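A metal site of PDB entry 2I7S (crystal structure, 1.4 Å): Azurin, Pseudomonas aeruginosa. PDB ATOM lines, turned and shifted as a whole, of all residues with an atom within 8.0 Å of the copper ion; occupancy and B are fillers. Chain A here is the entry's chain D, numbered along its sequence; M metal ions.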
ATOM      1  N   GLY A   9      -1.077  14.948   2.592  1.00  0.00           N
ATOM      2  CA  GLY A   9      -2.513  15.222   2.595  1.00  0.00           C
ATOM      3  C   GLY A   9      -2.790  16.416   1.694  1.00  0.00           C
ATOM      4  O   GLY A   9      -2.113  17.439   1.824  1.00  0.00           O
ATOM      5  N   ASN A  10      -3.774  16.301   0.814  1.00  0.00           N
ATOM      6  CA  ASN A  10      -3.928  17.285  -0.270  1.00  0.00           C
ATOM      7  C   ASN A  10      -5.113  18.183  -0.073  1.00  0.00           C
ATOM      8  O   ASN A  10      -5.726  18.262   1.002  1.00  0.00           O
ATOM      9  CB  ASN A  10      -3.993  16.548  -1.612  1.00  0.00           C
ATOM     10  CG  ASN A  10      -5.210  15.683  -1.827  1.00  0.00           C
ATOM     11  OD1 ASN A  10      -6.211  15.722  -1.095  1.00  0.00           O
ATOM     12  ND2 ASN A  10      -5.168  14.868  -2.875  1.00  0.00           N
ATOM     13  N   MET A  13      -8.787  16.597   0.830  1.00  0.00           N
ATOM     14  CA  MET A  13      -8.870  15.790   2.043  1.00  0.00           C
ATOM     15  C   MET A  13      -8.562  14.324   1.781  1.00  0.00           C
ATOM     16  O   MET A  13      -9.315  13.416   2.147  1.00  0.00           O
ATOM     17  CB  MET A  13     -10.258  15.853   2.727  1.00  0.00           C
ATOM     18  CG  MET A  13     -10.474  17.049   3.634  1.00  0.00           C
ATOM     19  SD  MET A  13     -12.230  17.374   3.912  1.00  0.00           S
ATOM     20  CE  MET A  13     -12.770  17.405   2.185  1.00  0.00           C
ATOM     21  N   GLN A  14      -7.439  14.100   1.129  1.00  0.00           N
ATOM     22  CA  GLN A  14      -7.037  12.721   0.873  1.00  0.00           C
ATOM     23  C   GLN A  14      -5.628  12.495   1.417  1.00  0.00           C
ATOM     24  O   GLN A  14      -4.762  13.291   1.045  1.00  0.00           O
ATOM     25  CB  GLN A  14      -7.052  12.395  -0.629  1.00  0.00           C
ATOM     26  CG  GLN A  14      -8.448  12.450  -1.234  1.00  0.00           C
ATOM     27  CD  GLN A  14      -8.444  12.614  -2.742  1.00  0.00           C
ATOM     28  OE1 GLN A  14      -7.576  13.247  -3.355  1.00  0.00           O
ATOM     29  NE2 GLN A  14      -9.466  12.005  -3.348  1.00  0.00           N
ATOM     30  N   PHE A  15      -5.423  11.454   2.214  1.00  0.00           N
ATOM     31  CA  PHE A  15      -4.091  10.955   2.506  1.00  0.00           C
ATOM     32  C   PHE A  15      -3.681  10.114   1.292  1.00  0.00           C
ATOM     33  O   PHE A  15      -4.560   9.671   0.522  1.00  0.00           O
ATOM     34  CB  PHE A  15      -4.033  10.121   3.784  1.00  0.00           C
ATOM     35  CG  PHE A  15      -3.920  10.875   5.107  1.00  0.00           C
ATOM     36  CD1 PHE A  15      -3.067  11.958   5.278  1.00  0.00           C
ATOM     37  CD2 PHE A  15      -4.696  10.473   6.175  1.00  0.00           C
ATOM     38  CE1 PHE A  15      -2.960  12.609   6.506  1.00  0.00           C
ATOM     39  CE2 PHE A  15      -4.597  11.121   7.392  1.00  0.00           C
ATOM     40  CZ  PHE A  15      -3.763  12.189   7.580  1.00  0.00           C
ATOM     41  N   LEU A  33       5.181  14.116   7.443  1.00  0.00           N
ATOM     42  CA  LEU A  33       3.970  14.701   6.894  1.00  0.00           C
ATOM     43  C   LEU A  33       4.219  15.945   6.050  1.00  0.00           C
ATOM     44  O   LEU A  33       4.865  16.878   6.517  1.00  0.00           O
ATOM     45  CB  LEU A  33       3.002  15.075   8.036  1.00  0.00           C
ATOM     46  CG  LEU A  33       1.603  15.568   7.579  1.00  0.00           C
ATOM     47  CD1 LEU A  33       0.891  14.477   6.818  1.00  0.00           C
ATOM     48  CD2 LEU A  33       0.839  16.056   8.804  1.00  0.00           C
ATOM     49  N   HIS A  35       2.154  18.521   2.697  1.00  0.00           N
ATOM     50  CA  HIS A  35       0.854  18.944   2.170  1.00  0.00           C
ATOM     51  C   HIS A  35       1.037  19.543   0.769  1.00  0.00           C
ATOM     52  O   HIS A  35       1.337  20.736   0.695  1.00  0.00           O
ATOM     53  CB  HIS A  35       0.208  19.968   3.073  1.00  0.00           C
ATOM     54  CG  HIS A  35      -1.191  20.420   2.804  1.00  0.00           C
ATOM     55  ND1 HIS A  35      -1.808  20.589   1.593  1.00  0.00           N
ATOM     56  CD2 HIS A  35      -2.134  20.752   3.731  1.00  0.00           C
ATOM     57  CE1 HIS A  35      -3.071  21.004   1.771  1.00  0.00           C
ATOM     58  NE2 HIS A  35      -3.275  21.110   3.066  1.00  0.00           N
ATOM     59  N   LYS A  41      -3.803  26.373   6.394  1.00  0.00           N
ATOM     60  CA  LYS A  41      -4.158  25.487   7.496  1.00  0.00           C
ATOM     61  C   LYS A  41      -5.461  25.823   8.216  1.00  0.00           C
ATOM     62  O   LYS A  41      -6.089  24.913   8.771  1.00  0.00           O
ATOM     63  CB  LYS A  41      -3.044  25.385   8.541  1.00  0.00           C
ATOM     64  CG  LYS A  41      -2.980  26.454   9.616  1.00  0.00           C
ATOM     65  CD  LYS A  41      -1.765  26.158  10.503  1.00  0.00           C
ATOM     66  CE  LYS A  41      -1.637  27.118  11.692  1.00  0.00           C
ATOM     67  NZ  LYS A  41      -0.276  26.952  12.319  1.00  0.00           N
ATOM     68  N   VAL A  43      -8.253  26.473   6.848  1.00  0.00           N
ATOM     69  CA  VAL A  43      -9.361  25.866   6.114  1.00  0.00           C
ATOM     70  C   VAL A  43      -9.040  24.486   5.579  1.00  0.00           C
ATOM     71  O   VAL A  43      -9.974  23.813   5.188  1.00  0.00           O
ATOM     72  CB  VAL A  43      -9.849  26.753   4.940  1.00  0.00           C
ATOM     73  CG1 VAL A  43     -10.551  27.991   5.482  1.00  0.00           C
ATOM     74  CG2 VAL A  43      -8.698  27.100   4.016  1.00  0.00           C
ATOM     75  N   MET A  44      -7.783  24.060   5.523  1.00  0.00           N
ATOM     76  CA  MET A  44      -7.403  22.762   4.986  1.00  0.00           C
ATOM     77  C   MET A  44      -6.182  22.232   5.747  1.00  0.00           C
ATOM     78  O   MET A  44      -5.323  21.593   5.119  1.00  0.00           O
ATOM     79  CB  MET A  44      -7.113  22.790   3.488  1.00  0.00           C
ATOM     80  CG  MET A  44      -6.955  21.462   2.782  1.00  0.00           C
ATOM     81  SD  MET A  44      -8.307  20.296   2.952  1.00  0.00           S
ATOM     82  CE  MET A  44      -9.666  21.254   2.334  1.00  0.00           C
ATOM     83  N   GLY A  45      -6.167  22.481   7.046  1.00  0.00           N
ATOM     84  CA  GLY A  45      -5.110  21.971   7.936  1.00  0.00           C
ATOM     85  C   GLY A  45      -5.110  20.459   8.050  1.00  0.00           C
ATOM     86  O   GLY A  45      -6.176  19.813   8.088  1.00  0.00           O
ATOM     87  N   HIS A  46      -3.915  19.868   8.094  1.00  0.00           N
ATOM     88  CA  HIS A  46      -3.767  18.428   8.262  1.00  0.00           C
ATOM     89  C   HIS A  46      -2.739  18.152   9.372  1.00  0.00           C
ATOM     90  O   HIS A  46      -1.709  18.793   9.447  1.00  0.00           O
ATOM     91  CB  HIS A  46      -3.400  17.666   7.017  1.00  0.00           C
ATOM     92  CG  HIS A  46      -4.302  17.787   5.844  1.00  0.00           C
ATOM     93  ND1 HIS A  46      -5.667  17.783   5.911  1.00  0.00           N
ATOM     94  CD2 HIS A  46      -4.002  17.935   4.513  1.00  0.00           C
ATOM     95  CE1 HIS A  46      -6.204  17.920   4.692  1.00  0.00           C
ATOM     96  NE2 HIS A  46      -5.184  18.014   3.820  1.00  0.00           N
ATOM     97  N   ASN A  47      -3.054  17.195  10.234  1.00  0.00           N
ATOM     98  CA  ASN A  47      -2.101  16.570  11.151  1.00  0.00           C
ATOM     99  C   ASN A  47      -2.152  15.055  10.896  1.00  0.00           C
ATOM    100  O   ASN A  47      -2.977  14.537  10.122  1.00  0.00           O
ATOM    101  CB  ASN A  47      -2.334  16.960  12.606  1.00  0.00           C
ATOM    102  CG  ASN A  47      -3.736  16.737  13.132  1.00  0.00           C
ATOM    103  OD1 ASN A  47      -4.425  15.918  12.544  1.00  0.00           O
ATOM    104  ND2 ASN A  47      -4.150  17.389  14.215  1.00  0.00           N
ATOM    105  N   TRP A  48      -1.226  14.309  11.491  1.00  0.00           N
ATOM    106  CA  TRP A  48      -1.209  12.850  11.480  1.00  0.00           C
ATOM    107  C   TRP A  48      -1.206  12.406  12.946  1.00  0.00           C
ATOM    108  O   TRP A  48      -0.281  12.756  13.687  1.00  0.00           O
ATOM    109  CB  TRP A  48      -0.016  12.295  10.709  1.00  0.00           C
ATOM    110  CG  TRP A  48       0.030  10.812  10.572  1.00  0.00           C
ATOM    111  CD1 TRP A  48      -0.461  10.102   9.487  1.00  0.00           C
ATOM    112  CD2 TRP A  48       0.569   9.843  11.458  1.00  0.00           C
ATOM    113  NE1 TRP A  48      -0.232   8.762   9.693  1.00  0.00           N
ATOM    114  CE2 TRP A  48       0.401   8.568  10.918  1.00  0.00           C
ATOM    115  CE3 TRP A  48       1.203   9.916  12.723  1.00  0.00           C
ATOM    116  CZ2 TRP A  48       0.808   7.379  11.520  1.00  0.00           C
ATOM    117  CZ3 TRP A  48       1.610   8.734  13.332  1.00  0.00           C
ATOM    118  CH2 TRP A  48       1.424   7.479  12.754  1.00  0.00           C
ATOM    119  N   TYR A  72      -5.984  21.287  16.989  1.00  0.00           N
ATOM    120  CA  TYR A  72      -7.187  20.471  17.057  1.00  0.00           C
ATOM    121  C   TYR A  72      -6.919  19.177  17.828  1.00  0.00           C
ATOM    122  O   TYR A  72      -7.408  18.111  17.472  1.00  0.00           O
ATOM    123  CB  TYR A  72      -7.738  20.182  15.646  1.00  0.00           C
ATOM    124  CG  TYR A  72      -8.512  21.394  15.104  1.00  0.00           C
ATOM    125  CD1 TYR A  72      -9.646  21.887  15.733  1.00  0.00           C
ATOM    126  CD2 TYR A  72      -8.016  22.020  13.970  1.00  0.00           C
ATOM    127  CE1 TYR A  72     -10.345  22.994  15.271  1.00  0.00           C
ATOM    128  CE2 TYR A  72      -8.716  23.129  13.490  1.00  0.00           C
ATOM    129  CZ  TYR A  72      -9.827  23.594  14.121  1.00  0.00           C
ATOM    130  OH  TYR A  72     -10.507  24.702  13.611  1.00  0.00           O
ATOM    131  N   LEU A  86      -0.451  20.593  13.351  1.00  0.00           N
ATOM    132  CA  LEU A  86      -1.308  20.913  12.193  1.00  0.00           C
ATOM    133  C   LEU A  86      -0.563  21.726  11.133  1.00  0.00           C
ATOM    134  O   LEU A  86       0.016  22.754  11.520  1.00  0.00           O
ATOM    135  CB  LEU A  86      -2.535  21.664  12.716  1.00  0.00           C
ATOM    136  CG  LEU A  86      -3.678  21.804  11.689  1.00  0.00           C
ATOM    137  CD1 LEU A  86      -4.490  20.513  11.626  1.00  0.00           C
ATOM    138  CD2 LEU A  86      -4.562  22.997  11.990  1.00  0.00           C
ATOM    139  N   ILE A  87      -0.566  21.318   9.867  1.00  0.00           N
ATOM    140  CA  ILE A  87       0.164  21.991   8.773  1.00  0.00           C
ATOM    141  C   ILE A  87      -0.794  22.391   7.657  1.00  0.00           C
ATOM    142  O   ILE A  87      -1.892  21.859   7.516  1.00  0.00           O
ATOM    143  CB  ILE A  87       1.274  21.119   8.189  1.00  0.00           C
ATOM    144  CG1 ILE A  87       0.824  19.811   7.531  1.00  0.00           C
ATOM    145  CG2 ILE A  87       2.370  20.813   9.211  1.00  0.00           C
ATOM    146  CD1 ILE A  87       1.896  19.164   6.667  1.00  0.00           C
ATOM    147  N   PHE A 111      -5.162   9.315  11.571  1.00  0.00           N
ATOM    148  CA  PHE A 111      -6.190  10.202  11.071  1.00  0.00           C
ATOM    149  C   PHE A 111      -5.796  11.677  11.207  1.00  0.00           C
ATOM    150  O   PHE A 111      -4.850  12.002  11.916  1.00  0.00           O
ATOM    151  CB  PHE A 111      -7.520   9.930  11.810  1.00  0.00           C
ATOM    152  CG  PHE A 111      -7.372   9.832  13.319  1.00  0.00           C
ATOM    153  CD1 PHE A 111      -7.510  10.938  14.132  1.00  0.00           C
ATOM    154  CD2 PHE A 111      -7.057   8.596  13.883  1.00  0.00           C
ATOM    155  CE1 PHE A 111      -7.355  10.826  15.517  1.00  0.00           C
ATOM    156  CE2 PHE A 111      -6.929   8.475  15.263  1.00  0.00           C
ATOM    157  CZ  PHE A 111      -7.061   9.593  16.077  1.00  0.00           C
ATOM    158  N   CYS A 112      -6.536  12.554  10.536  1.00  0.00           N
ATOM    159  CA  CYS A 112      -6.420  14.000  10.734  1.00  0.00           C
ATOM    160  C   CYS A 112      -7.550  14.476  11.646  1.00  0.00           C
ATOM    161  O   CYS A 112      -8.712  14.083  11.416  1.00  0.00           O
ATOM    162  CB  CYS A 112      -6.470  14.731   9.378  1.00  0.00           C
ATOM    163  SG  CYS A 112      -6.455  16.523   9.537  1.00  0.00           S
ATOM    164  N   THR A 113      -7.250  15.304  12.621  1.00  0.00           N
ATOM    165  CA  THR A 113      -8.303  15.796  13.528  1.00  0.00           C
ATOM    166  C   THR A 113      -8.848  17.198  13.215  1.00  0.00           C
ATOM    167  O   THR A 113      -9.672  17.734  13.966  1.00  0.00           O
ATOM    168  CB  THR A 113      -7.859  15.810  15.016  1.00  0.00           C
ATOM    169  OG1 THR A 113      -6.799  16.750  15.172  1.00  0.00           O
ATOM    170  CG2 THR A 113      -7.372  14.438  15.464  1.00  0.00           C
ATOM    171  N   PHE A 114      -8.449  17.794  12.084  1.00  0.00           N
ATOM    172  CA  PHE A 114      -9.063  19.054  11.658  1.00  0.00           C
ATOM    173  C   PHE A 114     -10.574  18.757  11.483  1.00  0.00           C
ATOM    174  O   PHE A 114     -10.920  17.699  10.933  1.00  0.00           O
ATOM    175  CB  PHE A 114      -8.470  19.523  10.324  1.00  0.00           C
ATOM    176  CG  PHE A 114      -8.972  20.903   9.866  1.00  0.00           C
ATOM    177  CD1 PHE A 114     -10.198  21.025   9.214  1.00  0.00           C
ATOM    178  CD2 PHE A 114      -8.249  22.065  10.081  1.00  0.00           C
ATOM    179  CE1 PHE A 114     -10.687  22.276   8.832  1.00  0.00           C
ATOM    180  CE2 PHE A 114      -8.731  23.312   9.703  1.00  0.00           C
ATOM    181  CZ  PHE A 114      -9.955  23.425   9.062  1.00  0.00           C
ATOM    182  N   PRO A 115     -11.501  19.607  11.908  1.00  0.00           N
ATOM    183  CA  PRO A 115     -12.940  19.305  11.879  1.00  0.00           C
ATOM    184  C   PRO A 115     -13.467  18.808  10.541  1.00  0.00           C
ATOM    185  O   PRO A 115     -13.307  19.487   9.526  1.00  0.00           O
ATOM    186  CB  PRO A 115     -13.591  20.635  12.298  1.00  0.00           C
ATOM    187  CG  PRO A 115     -12.560  21.199  13.236  1.00  0.00           C
ATOM    188  CD  PRO A 115     -11.244  20.911  12.538  1.00  0.00           C
ATOM    189  N   GLY A 116     -14.065  17.602  10.581  1.00  0.00           N
ATOM    190  CA  GLY A 116     -14.605  16.993   9.392  1.00  0.00           C
ATOM    191  C   GLY A 116     -13.666  16.083   8.635  1.00  0.00           C
ATOM    192  O   GLY A 116     -14.119  15.201   7.893  1.00  0.00           O
ATOM    193  N   HIS A 117     -12.339  16.267   8.819  1.00  0.00           N
ATOM    194  CA  HIS A 117     -11.408  15.567   7.907  1.00  0.00           C
ATOM    195  C   HIS A 117     -11.372  14.061   8.152  1.00  0.00           C
ATOM    196  O   HIS A 117     -11.086  13.300   7.197  1.00  0.00           O
ATOM    197  CB  HIS A 117      -9.991  16.155   7.986  1.00  0.00           C
ATOM    198  CG  HIS A 117      -9.899  17.499   7.346  1.00  0.00           C
ATOM    199  ND1 HIS A 117      -8.705  18.169   7.110  1.00  0.00           N
ATOM    200  CD2 HIS A 117     -10.899  18.299   6.871  1.00  0.00           C
ATOM    201  CE1 HIS A 117      -9.002  19.325   6.532  1.00  0.00           C
ATOM    202  NE2 HIS A 117     -10.339  19.430   6.363  1.00  0.00           N
ATOM    203  N   SER A 118     -11.646  13.596   9.362  1.00  0.00           N
ATOM    204  CA  SER A 118     -11.379  12.184   9.670  1.00  0.00           C
ATOM    205  C   SER A 118     -12.394  11.273   8.985  1.00  0.00           C
ATOM    206  O   SER A 118     -12.201  10.072   8.857  1.00  0.00           O
ATOM    207  CB  SER A 118     -11.386  11.964  11.196  1.00  0.00           C
ATOM    208  OG  SER A 118     -12.607  12.395  11.726  1.00  0.00           O
ATOM    209  N   MET A 121      -9.999  11.174   5.803  1.00  0.00           N
ATOM    210  CA  MET A 121      -8.591  11.119   6.147  1.00  0.00           C
ATOM    211  C   MET A 121      -8.321  10.221   7.347  1.00  0.00           C
ATOM    212  O   MET A 121      -8.097  10.707   8.477  1.00  0.00           O
ATOM    213  CB  MET A 121      -8.082  12.532   6.357  1.00  0.00           C
ATOM    214  CG  MET A 121      -8.253  13.428   5.144  1.00  0.00           C
ATOM    215  SD  MET A 121      -7.402  15.011   5.311  1.00  0.00           S
ATOM    216  CE  MET A 121      -5.689  14.529   5.110  1.00  0.00           C
HETATM  217 CU    CU M   1      -6.832  17.579   7.562  1.00  0.00          CU
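The side-chain sulfur (SD) of Met 13 lies close to a ring nitrogen (NE2) of His 117 (3.7 Å). A ring nitrogen (ND1) of His 46 sits close to the side-chain sulfur (SD) of Met 121, at 3.3 Å. The backbone carbonyl oxygen (O) of His 46 sits at hydrogen-bond distance from the backbone NH (N) of Ile 87, at 2.8 Å. O of Asn 10 is in hydrogen-bond range of NE2 of His 46 (2.9 Å). The backbone carbonyl oxygen of Met 121 sits at hydrogen-bond distance from the backbone NH of Cys 112. The side-chain sulfur of Cys 112 lies close to the backbone NH of Phe 114 (3.5 Å). SG of Cys 112 sits close to N of Asn 47.
Phe 114 touches the copper ion. Met 121 touches the copper ion (SD to CU, 3.5 Å). Within 4 Å of the copper ion: Gly 45, His 46, Cys 112, Phe 114, His 117 and Met 121. Along chain A the residues within 4 Å of the copper ion span positions 45 to 121.
ND1 of His 117 is bound to the copper ion, at 2.0 Å. ND1 of His 46 binds the copper ion (2.0 Å). The copper ion is bound by the side-chain sulfur (SG) of Cys 112 (2.3 Å). The copper ion is bound by O of Gly 45 (2.4 Å). The copper ion has four donor atoms within binding distance.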
